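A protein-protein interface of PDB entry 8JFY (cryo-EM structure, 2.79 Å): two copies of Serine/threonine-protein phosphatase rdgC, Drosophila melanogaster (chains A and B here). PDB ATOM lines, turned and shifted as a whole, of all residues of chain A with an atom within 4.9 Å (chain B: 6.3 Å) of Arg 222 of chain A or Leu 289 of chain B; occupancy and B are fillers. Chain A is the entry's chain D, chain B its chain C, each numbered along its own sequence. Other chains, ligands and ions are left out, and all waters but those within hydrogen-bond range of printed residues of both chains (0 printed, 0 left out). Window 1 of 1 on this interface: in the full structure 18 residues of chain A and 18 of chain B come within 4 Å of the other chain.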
ATOM      1  N   VAL A 218     -18.254 -18.309 -19.645  1.00  0.00           N
ATOM      2  CA  VAL A 218     -19.358 -19.246 -19.461  1.00  0.00           C
ATOM      3  C   VAL A 218     -20.618 -18.502 -19.041  1.00  0.00           C
ATOM      4  O   VAL A 218     -21.716 -18.783 -19.539  1.00  0.00           O
ATOM      5  CB  VAL A 218     -18.971 -20.330 -18.439  1.00  0.00           C
ATOM      6  CG1 VAL A 218     -20.143 -21.268 -18.186  1.00  0.00           C
ATOM      7  CG2 VAL A 218     -17.754 -21.105 -18.923  1.00  0.00           C
ATOM      8  N   MET A 219     -20.485 -17.538 -18.126  1.00  0.00           N
ATOM      9  CA  MET A 219     -21.630 -16.731 -17.723  1.00  0.00           C
ATOM     10  C   MET A 219     -22.162 -15.904 -18.888  1.00  0.00           C
ATOM     11  O   MET A 219     -23.380 -15.748 -19.041  1.00  0.00           O
ATOM     12  CB  MET A 219     -21.246 -15.823 -16.554  1.00  0.00           C
ATOM     13  CG  MET A 219     -21.483 -16.435 -15.184  1.00  0.00           C
ATOM     14  SD  MET A 219     -23.138 -17.127 -15.000  1.00  0.00           S
ATOM     15  CE  MET A 219     -23.685 -16.294 -13.513  1.00  0.00           C
ATOM     16  N   ASN A 220     -21.262 -15.361 -19.713  1.00  0.00           N
ATOM     17  CA  ASN A 220     -21.691 -14.599 -20.882  1.00  0.00           C
ATOM     18  C   ASN A 220     -22.472 -15.464 -21.861  1.00  0.00           C
ATOM     19  O   ASN A 220     -23.492 -15.022 -22.403  1.00  0.00           O
ATOM     20  CB  ASN A 220     -20.479 -13.975 -21.576  1.00  0.00           C
ATOM     21  CG  ASN A 220     -19.851 -12.861 -20.763  1.00  0.00           C
ATOM     22  OD1 ASN A 220     -20.252 -12.603 -19.628  1.00  0.00           O
ATOM     23  ND2 ASN A 220     -18.853 -12.200 -21.337  1.00  0.00           N
ATOM     24  N   ALA A 221     -22.011 -16.693 -22.103  1.00  0.00           N
ATOM     25  CA  ALA A 221     -22.752 -17.606 -22.967  1.00  0.00           C
ATOM     26  C   ALA A 221     -24.090 -17.998 -22.350  1.00  0.00           C
ATOM     27  O   ALA A 221     -25.090 -18.131 -23.064  1.00  0.00           O
ATOM     28  CB  ALA A 221     -21.914 -18.852 -23.257  1.00  0.00           C
ATOM     29  N   ARG A 222     -24.121 -18.190 -21.028  1.00  0.00           N
ATOM     30  CA  ARG A 222     -25.363 -18.546 -20.351  1.00  0.00           C
ATOM     31  C   ARG A 222     -26.398 -17.432 -20.444  1.00  0.00           C
ATOM     32  O   ARG A 222     -27.582 -17.705 -20.674  1.00  0.00           O
ATOM     33  CB  ARG A 222     -25.073 -18.888 -18.887  1.00  0.00           C
ATOM     34  CG  ARG A 222     -26.303 -19.000 -17.998  1.00  0.00           C
ATOM     35  CD  ARG A 222     -27.225 -20.125 -18.438  1.00  0.00           C
ATOM     36  NE  ARG A 222     -28.415 -20.205 -17.600  1.00  0.00           N
ATOM     37  CZ  ARG A 222     -29.509 -19.477 -17.780  1.00  0.00           C
ATOM     38  NH1 ARG A 222     -29.602 -18.601 -18.767  1.00  0.00           N
ATOM     39  NH2 ARG A 222     -30.534 -19.630 -16.947  1.00  0.00           N
ATOM     40  N   TYR A 223     -25.979 -16.179 -20.276  1.00  0.00           N
ATOM     41  CA  TYR A 223     -26.898 -15.049 -20.278  1.00  0.00           C
ATOM     42  C   TYR A 223     -26.952 -14.312 -21.610  1.00  0.00           C
ATOM     43  O   TYR A 223     -27.667 -13.310 -21.718  1.00  0.00           O
ATOM     44  CB  TYR A 223     -26.535 -14.073 -19.154  1.00  0.00           C
ATOM     45  CG  TYR A 223     -26.944 -14.565 -17.785  1.00  0.00           C
ATOM     46  CD1 TYR A 223     -28.250 -14.415 -17.334  1.00  0.00           C
ATOM     47  CD2 TYR A 223     -26.031 -15.192 -16.947  1.00  0.00           C
ATOM     48  CE1 TYR A 223     -28.632 -14.869 -16.086  1.00  0.00           C
ATOM     49  CE2 TYR A 223     -26.404 -15.650 -15.699  1.00  0.00           C
ATOM     50  CZ  TYR A 223     -27.706 -15.485 -15.272  1.00  0.00           C
ATOM     51  OH  TYR A 223     -28.080 -15.938 -14.028  1.00  0.00           O
ATOM     52  N   GLY A 224     -26.221 -14.772 -22.621  1.00  0.00           N
ATOM     53  CA  GLY A 224     -26.337 -14.222 -23.956  1.00  0.00           C
ATOM     54  C   GLY A 224     -25.580 -12.942 -24.218  1.00  0.00           C
ATOM     55  O   GLY A 224     -25.942 -12.214 -25.151  1.00  0.00           O
ATOM     56  N   ILE A 226     -22.539 -12.771 -25.369  1.00  0.00           N
ATOM     57  CA  ILE A 226     -21.857 -12.974 -26.644  1.00  0.00           C
ATOM     58  C   ILE A 226     -22.807 -12.737 -27.809  1.00  0.00           C
ATOM     59  O   ILE A 226     -22.398 -12.219 -28.855  1.00  0.00           O
ATOM     60  CB  ILE A 226     -21.217 -14.377 -26.694  1.00  0.00           C
ATOM     61  CG1 ILE A 226     -22.287 -15.474 -26.675  1.00  0.00           C
ATOM     62  CG2 ILE A 226     -20.242 -14.561 -25.539  1.00  0.00           C
ATOM     63  CD1 ILE A 226     -21.734 -16.868 -26.853  1.00  0.00           C
ATOM     64  N   ARG A 227     -24.083 -13.098 -27.655  1.00  0.00           N
ATOM     65  CA  ARG A 227     -25.065 -12.783 -28.687  1.00  0.00           C
ATOM     66  C   ARG A 227     -25.265 -11.280 -28.838  1.00  0.00           C
ATOM     67  O   ARG A 227     -25.414 -10.791 -29.963  1.00  0.00           O
ATOM     68  CB  ARG A 227     -26.402 -13.464 -28.383  1.00  0.00           C
ATOM     69  CG  ARG A 227     -26.626 -14.747 -29.172  1.00  0.00           C
ATOM     70  CD  ARG A 227     -27.637 -15.664 -28.500  1.00  0.00           C
ATOM     71  NE  ARG A 227     -26.996 -16.686 -27.680  1.00  0.00           N
ATOM     72  CZ  ARG A 227     -27.279 -16.907 -26.404  1.00  0.00           C
ATOM     73  NH1 ARG A 227     -28.208 -16.209 -25.771  1.00  0.00           N
ATOM     74  NH2 ARG A 227     -26.621 -17.858 -25.747  1.00  0.00           N
ATOM     75  N   ASN B 213     -32.879 -28.804 -20.772  1.00  0.00           N
ATOM     76  CA  ASN B 213     -32.035 -27.615 -20.762  1.00  0.00           C
ATOM     77  C   ASN B 213     -30.691 -27.860 -20.087  1.00  0.00           C
ATOM     78  O   ASN B 213     -29.714 -27.183 -20.420  1.00  0.00           O
ATOM     79  CB  ASN B 213     -32.760 -26.459 -20.070  1.00  0.00           C
ATOM     80  CG  ASN B 213     -32.889 -26.663 -18.574  1.00  0.00           C
ATOM     81  OD1 ASN B 213     -33.495 -27.632 -18.118  1.00  0.00           O
ATOM     82  ND2 ASN B 213     -32.319 -25.747 -17.802  1.00  0.00           N
ATOM     83  N   ASP B 216     -26.304 -29.731 -21.512  1.00  0.00           N
ATOM     84  CA  ASP B 216     -25.482 -28.775 -22.241  1.00  0.00           C
ATOM     85  C   ASP B 216     -24.093 -28.739 -21.624  1.00  0.00           C
ATOM     86  O   ASP B 216     -23.956 -28.824 -20.400  1.00  0.00           O
ATOM     87  CB  ASP B 216     -26.111 -27.376 -22.212  1.00  0.00           C
ATOM     88  CG  ASP B 216     -26.149 -26.728 -23.578  1.00  0.00           C
ATOM     89  OD1 ASP B 216     -25.295 -27.072 -24.420  1.00  0.00           O
ATOM     90  OD2 ASP B 216     -27.031 -25.875 -23.810  1.00  0.00           O
ATOM     91  N   VAL B 218     -22.146 -26.106 -21.610  1.00  0.00           N
ATOM     92  CA  VAL B 218     -22.122 -24.869 -20.835  1.00  0.00           C
ATOM     93  C   VAL B 218     -22.830 -25.069 -19.500  1.00  0.00           C
ATOM     94  O   VAL B 218     -22.350 -24.617 -18.453  1.00  0.00           O
ATOM     95  CB  VAL B 218     -22.747 -23.719 -21.644  1.00  0.00           C
ATOM     96  CG1 VAL B 218     -22.792 -22.445 -20.814  1.00  0.00           C
ATOM     97  CG2 VAL B 218     -21.972 -23.497 -22.933  1.00  0.00           C
ATOM     98  N   MET B 219     -23.977 -25.752 -19.513  1.00  0.00           N
ATOM     99  CA  MET B 219     -24.682 -26.047 -18.270  1.00  0.00           C
ATOM    100  C   MET B 219     -23.854 -26.956 -17.368  1.00  0.00           C
ATOM    101  O   MET B 219     -23.839 -26.778 -16.144  1.00  0.00           O
ATOM    102  CB  MET B 219     -26.036 -26.686 -18.575  1.00  0.00           C
ATOM    103  CG  MET B 219     -27.177 -25.692 -18.718  1.00  0.00           C
ATOM    104  SD  MET B 219     -27.263 -24.519 -17.353  1.00  0.00           S
ATOM    105  CE  MET B 219     -28.965 -24.729 -16.838  1.00  0.00           C
ATOM    106  N   ARG B 222     -21.275 -24.840 -15.780  1.00  0.00           N
ATOM    107  CA  ARG B 222     -21.902 -23.967 -14.794  1.00  0.00           C
ATOM    108  C   ARG B 222     -22.215 -24.708 -13.500  1.00  0.00           C
ATOM    109  O   ARG B 222     -21.998 -24.167 -12.409  1.00  0.00           O
ATOM    110  CB  ARG B 222     -23.174 -23.354 -15.382  1.00  0.00           C
ATOM    111  CG  ARG B 222     -24.075 -22.651 -14.376  1.00  0.00           C
ATOM    112  CD  ARG B 222     -23.386 -21.462 -13.728  1.00  0.00           C
ATOM    113  NE  ARG B 222     -24.245 -20.816 -12.743  1.00  0.00           N
ATOM    114  CZ  ARG B 222     -24.365 -21.206 -11.481  1.00  0.00           C
ATOM    115  NH1 ARG B 222     -23.690 -22.243 -11.012  1.00  0.00           N
ATOM    116  NH2 ARG B 222     -25.185 -20.543 -10.672  1.00  0.00           N
ATOM    117  N   SER B 287     -24.402 -27.752 -28.704  1.00  0.00           N
ATOM    118  CA  SER B 287     -24.664 -26.913 -27.544  1.00  0.00           C
ATOM    119  C   SER B 287     -25.710 -25.868 -27.905  1.00  0.00           C
ATOM    120  O   SER B 287     -25.633 -25.241 -28.968  1.00  0.00           O
ATOM    121  CB  SER B 287     -23.384 -26.230 -27.050  1.00  0.00           C
ATOM    122  OG  SER B 287     -23.675 -25.241 -26.079  1.00  0.00           O
ATOM    123  N   ILE B 288     -26.684 -25.682 -27.019  1.00  0.00           N
ATOM    124  CA  ILE B 288     -27.778 -24.750 -27.280  1.00  0.00           C
ATOM    125  C   ILE B 288     -27.390 -23.321 -26.927  1.00  0.00           C
ATOM    126  O   ILE B 288     -27.604 -22.401 -27.722  1.00  0.00           O
ATOM    127  CB  ILE B 288     -29.040 -25.199 -26.514  1.00  0.00           C
ATOM    128  CG1 ILE B 288     -29.586 -26.502 -27.100  1.00  0.00           C
ATOM    129  CG2 ILE B 288     -30.101 -24.109 -26.548  1.00  0.00           C
ATOM    130  CD1 ILE B 288     -30.627 -27.174 -26.232  1.00  0.00           C
ATOM    131  N   LEU B 289     -26.818 -23.110 -25.739  1.00  0.00           N
ATOM    132  CA  LEU B 289     -26.432 -21.763 -25.331  1.00  0.00           C
ATOM    133  C   LEU B 289     -25.310 -21.206 -26.198  1.00  0.00           C
ATOM    134  O   LEU B 289     -25.326 -20.018 -26.540  1.00  0.00           O
ATOM    135  CB  LEU B 289     -26.016 -21.758 -23.860  1.00  0.00           C
ATOM    136  CG  LEU B 289     -27.110 -22.085 -22.842  1.00  0.00           C
ATOM    137  CD1 LEU B 289     -26.533 -22.156 -21.437  1.00  0.00           C
ATOM    138  CD2 LEU B 289     -28.236 -21.066 -22.915  1.00  0.00           C
ATOM    139  N   ARG B 290     -24.336 -22.039 -26.562  1.00  0.00           N
ATOM    140  CA  ARG B 290     -23.193 -21.624 -27.376  1.00  0.00           C
ATOM    141  C   ARG B 290     -23.077 -22.565 -28.567  1.00  0.00           C
ATOM    142  O   ARG B 290     -22.324 -23.549 -28.525  1.00  0.00           O
ATOM    143  CB  ARG B 290     -21.903 -21.611 -26.553  1.00  0.00           C
ATOM    144  CG  ARG B 290     -20.722 -20.962 -27.258  1.00  0.00           C
ATOM    145  CD  ARG B 290     -19.413 -21.286 -26.556  1.00  0.00           C
ATOM    146  NE  ARG B 290     -19.365 -20.738 -25.206  1.00  0.00           N
ATOM    147  CZ  ARG B 290     -18.876 -19.544 -24.899  1.00  0.00           C
ATOM    148  NH1 ARG B 290     -18.380 -18.741 -25.827  1.00  0.00           N
ATOM    149  NH2 ARG B 290     -18.882 -19.146 -23.630  1.00  0.00           N
ATOM    150  N   PRO B 291     -23.817 -22.301 -29.640  1.00  0.00           N
ATOM    151  CA  PRO B 291     -23.727 -23.144 -30.839  1.00  0.00           C
ATOM    152  C   PRO B 291     -22.317 -23.140 -31.403  1.00  0.00           C
ATOM    153  O   PRO B 291     -21.629 -22.107 -31.371  1.00  0.00           O
ATOM    154  CB  PRO B 291     -24.720 -22.486 -31.809  1.00  0.00           C
ATOM    155  CG  PRO B 291     -25.678 -21.759 -30.922  1.00  0.00           C
ATOM    156  CD  PRO B 291     -24.849 -21.258 -29.777  1.00  0.00           C
ATOM    157  N   TRP B 304     -32.957 -21.494 -34.273  1.00  0.00           N
ATOM    158  CA  TRP B 304     -32.485 -21.636 -32.898  1.00  0.00           C
ATOM    159  C   TRP B 304     -33.536 -21.173 -31.896  1.00  0.00           C
ATOM    160  O   TRP B 304     -33.590 -21.679 -30.767  1.00  0.00           O
ATOM    161  CB  TRP B 304     -31.184 -20.855 -32.714  1.00  0.00           C
ATOM    162  CG  TRP B 304     -30.706 -20.797 -31.295  1.00  0.00           C
ATOM    163  CD1 TRP B 304     -30.083 -21.790 -30.598  1.00  0.00           C
ATOM    164  CD2 TRP B 304     -30.811 -19.683 -30.400  1.00  0.00           C
ATOM    165  NE1 TRP B 304     -29.794 -21.366 -29.323  1.00  0.00           N
ATOM    166  CE2 TRP B 304     -30.230 -20.075 -29.176  1.00  0.00           C
ATOM    167  CE3 TRP B 304     -31.339 -18.393 -30.513  1.00  0.00           C
ATOM    168  CZ2 TRP B 304     -30.164 -19.224 -28.075  1.00  0.00           C
ATOM    169  CZ3 TRP B 304     -31.272 -17.549 -29.419  1.00  0.00           C
ATOM    170  CH2 TRP B 304     -30.690 -17.969 -28.216  1.00  0.00           C
ATOM    171  N   PHE B 308     -34.757 -22.903 -28.379  1.00  0.00           N
ATOM    172  CA  PHE B 308     -34.583 -22.133 -27.152  1.00  0.00           C
ATOM    173  C   PHE B 308     -35.901 -21.985 -26.401  1.00  0.00           C
ATOM    174  O   PHE B 308     -35.943 -22.133 -25.173  1.00  0.00           O
ATOM    175  CB  PHE B 308     -33.992 -20.762 -27.489  1.00  0.00           C
ATOM    176  CG  PHE B 308     -33.381 -20.056 -26.314  1.00  0.00           C
ATOM    177  CD1 PHE B 308     -32.290 -20.597 -25.658  1.00  0.00           C
ATOM    178  CD2 PHE B 308     -33.890 -18.845 -25.878  1.00  0.00           C
ATOM    179  CE1 PHE B 308     -31.720 -19.947 -24.581  1.00  0.00           C
ATOM    180  CE2 PHE B 308     -33.323 -18.190 -24.800  1.00  0.00           C
ATOM    181  CZ  PHE B 308     -32.237 -18.741 -24.153  1.00  0.00           C
ATOM    182  N   TRP B 312     -36.565 -23.574 -22.713  1.00  0.00           N
ATOM    183  CA  TRP B 312     -36.438 -22.666 -21.580  1.00  0.00           C
ATOM    184  C   TRP B 312     -37.731 -21.980 -21.157  1.00  0.00           C
ATOM    185  O   TRP B 312     -37.703 -21.204 -20.197  1.00  0.00           O
ATOM    186  CB  TRP B 312     -35.388 -21.586 -21.885  1.00  0.00           C
ATOM    187  CG  TRP B 312     -33.977 -22.082 -21.790  1.00  0.00           C
ATOM    188  CD1 TRP B 312     -33.199 -22.537 -22.814  1.00  0.00           C
ATOM    189  CD2 TRP B 312     -33.175 -22.172 -20.607  1.00  0.00           C
ATOM    190  NE1 TRP B 312     -31.963 -22.905 -22.342  1.00  0.00           N
ATOM    191  CE2 TRP B 312     -31.923 -22.690 -20.989  1.00  0.00           C
ATOM    192  CE3 TRP B 312     -33.395 -21.865 -19.260  1.00  0.00           C
ATOM    193  CZ2 TRP B 312     -30.894 -22.909 -20.076  1.00  0.00           C
ATOM    194  CZ3 TRP B 312     -32.373 -22.082 -18.355  1.00  0.00           C
ATOM    195  CH2 TRP B 312     -31.138 -22.598 -18.766  1.00  0.00           C
ATOM    196  N   ARG B 327     -35.495 -16.376 -14.982  1.00  0.00           N
ATOM    197  CA  ARG B 327     -34.458 -17.290 -15.447  1.00  0.00           C
ATOM    198  C   ARG B 327     -33.468 -16.609 -16.381  1.00  0.00           C
ATOM    199  O   ARG B 327     -32.321 -17.055 -16.493  1.00  0.00           O
ATOM    200  CB  ARG B 327     -35.086 -18.493 -16.151  1.00  0.00           C
ATOM    201  CG  ARG B 327     -35.856 -19.431 -15.238  1.00  0.00           C
ATOM    202  CD  ARG B 327     -36.298 -20.678 -15.991  1.00  0.00           C
ATOM    203  NE  ARG B 327     -37.156 -21.535 -15.183  1.00  0.00           N
ATOM    204  CZ  ARG B 327     -36.712 -22.467 -14.350  1.00  0.00           C
ATOM    205  NH1 ARG B 327     -35.419 -22.688 -14.187  1.00  0.00           N
ATOM    206  NH2 ARG B 327     -37.590 -23.193 -13.664  1.00  0.00           N
ATOM    207  N   GLY B 328     -33.884 -15.537 -17.052  1.00  0.00           N
ATOM    208  CA  GLY B 328     -33.058 -14.920 -18.065  1.00  0.00           C
ATOM    209  C   GLY B 328     -33.069 -15.628 -19.398  1.00  0.00           C
ATOM    210  O   GLY B 328     -32.352 -15.207 -20.314  1.00  0.00           O
ATOM    211  N   ALA B 329     -33.859 -16.690 -19.536  1.00  0.00           N
ATOM    212  CA  ALA B 329     -33.933 -17.456 -20.769  1.00  0.00           C
ATOM    213  C   ALA B 329     -35.354 -17.971 -20.943  1.00  0.00           C
ATOM    214  O   ALA B 329     -36.032 -18.301 -19.966  1.00  0.00           O
ATOM    215  CB  ALA B 329     -32.938 -18.622 -20.765  1.00  0.00           C
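O of Ala 221 of chain A sits at hydrogen-bond distance from NH2 of Arg 227 of chain A (3.1 Å). The side-chain hydroxyl of Ser 287 of chain B sits close to the backbone carbonyl oxygen of Arg 290 of chain B (3.3 Å). OD2 of Asp 216 of chain B lies within hydrogen-bond range of N of Leu 289 of chain B (3.4 Å). O of Ile 288 of chain B lies within hydrogen-bond range of NE1 of Trp 304 of chain B (2.9 Å).
Val 218 of chain B touches its own counterpart, Val 218 of chain A. Positions printed for both chains: 218, 219 and 222. Of the 10 pairs that touch across the chains among the printed residues, 1 has its exchanged pair printed and touching as well.
CG1 of Val 218 of chain B touches CG1 of Val 218 of chain A, at 3.9 Å. CB of Leu 289 of chain B touches O of Ala 221 of chain A, 3.8 Å away. Arg 290 of chain B touches Ala 221 of chain A. Leu 289 of chain B touches Arg 222 of chain A (CD1 to CD, 3.7 Å). Trp 312 of chain B touches Arg 222 of chain A (CZ3 to NH2, 3.4 Å). Arg 222 of chain A touches Ala 329 of chain B. Arg 290 of chain B touches Ile 226 of chain A. Trp 304 of chain B touches Arg 227 of chain A (CH2 to CD, 3.8 Å).
Of the 9 printed residues of chain A, 5 touch a printed residue of chain B. Hydrophobic or aromatic side chains of chain A that line the printed part of chain B: Val 218, Ala 221 and Ile 226. Among the printed residues, no Asp or Glu carboxylate lies within 4 Å of a Lys or Arg side-chain nitrogen of the other chain.
The backbone carbonyl oxygen of Leu 289 of chain B lies within hydrogen-bond range of the guanidinium group of Arg 227 of chain A, at 2.6 Å. The backbone carbonyl oxygen (O) of Arg 327 of chain B lies within hydrogen-bond range of the guanidinium group (NH2) of Arg 222 of chain A, at 3.2 Å.
Arg 222 of chain A touches just these residues of chain B: Leu 289, Trp 312, Arg 327 and Ala 329. Printed residues of chain B within 4 Å of Ile 226 of chain A: Arg 290. Of the printed residues of chain A, Trp 312 of chain B touches Arg 222 (3.4 Å). Printed residues of chain A within 4 Å of Trp 304 of chain B: Arg 227. Printed residues of chain A within 4 Å of Arg 290 of chain B: Ala 221 and Ile 226. Of the printed residues of chain A, Arg 327 of chain B touches Arg 222 (3.2 Å). The nearest residue of chain A that does not touch Leu 289 of chain B is Ile 226 of chain A (4.8 Å). The nearest printed residue of chain B that does not touch Ile 226 of chain A is Leu 289 of chain B (4.8 Å).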
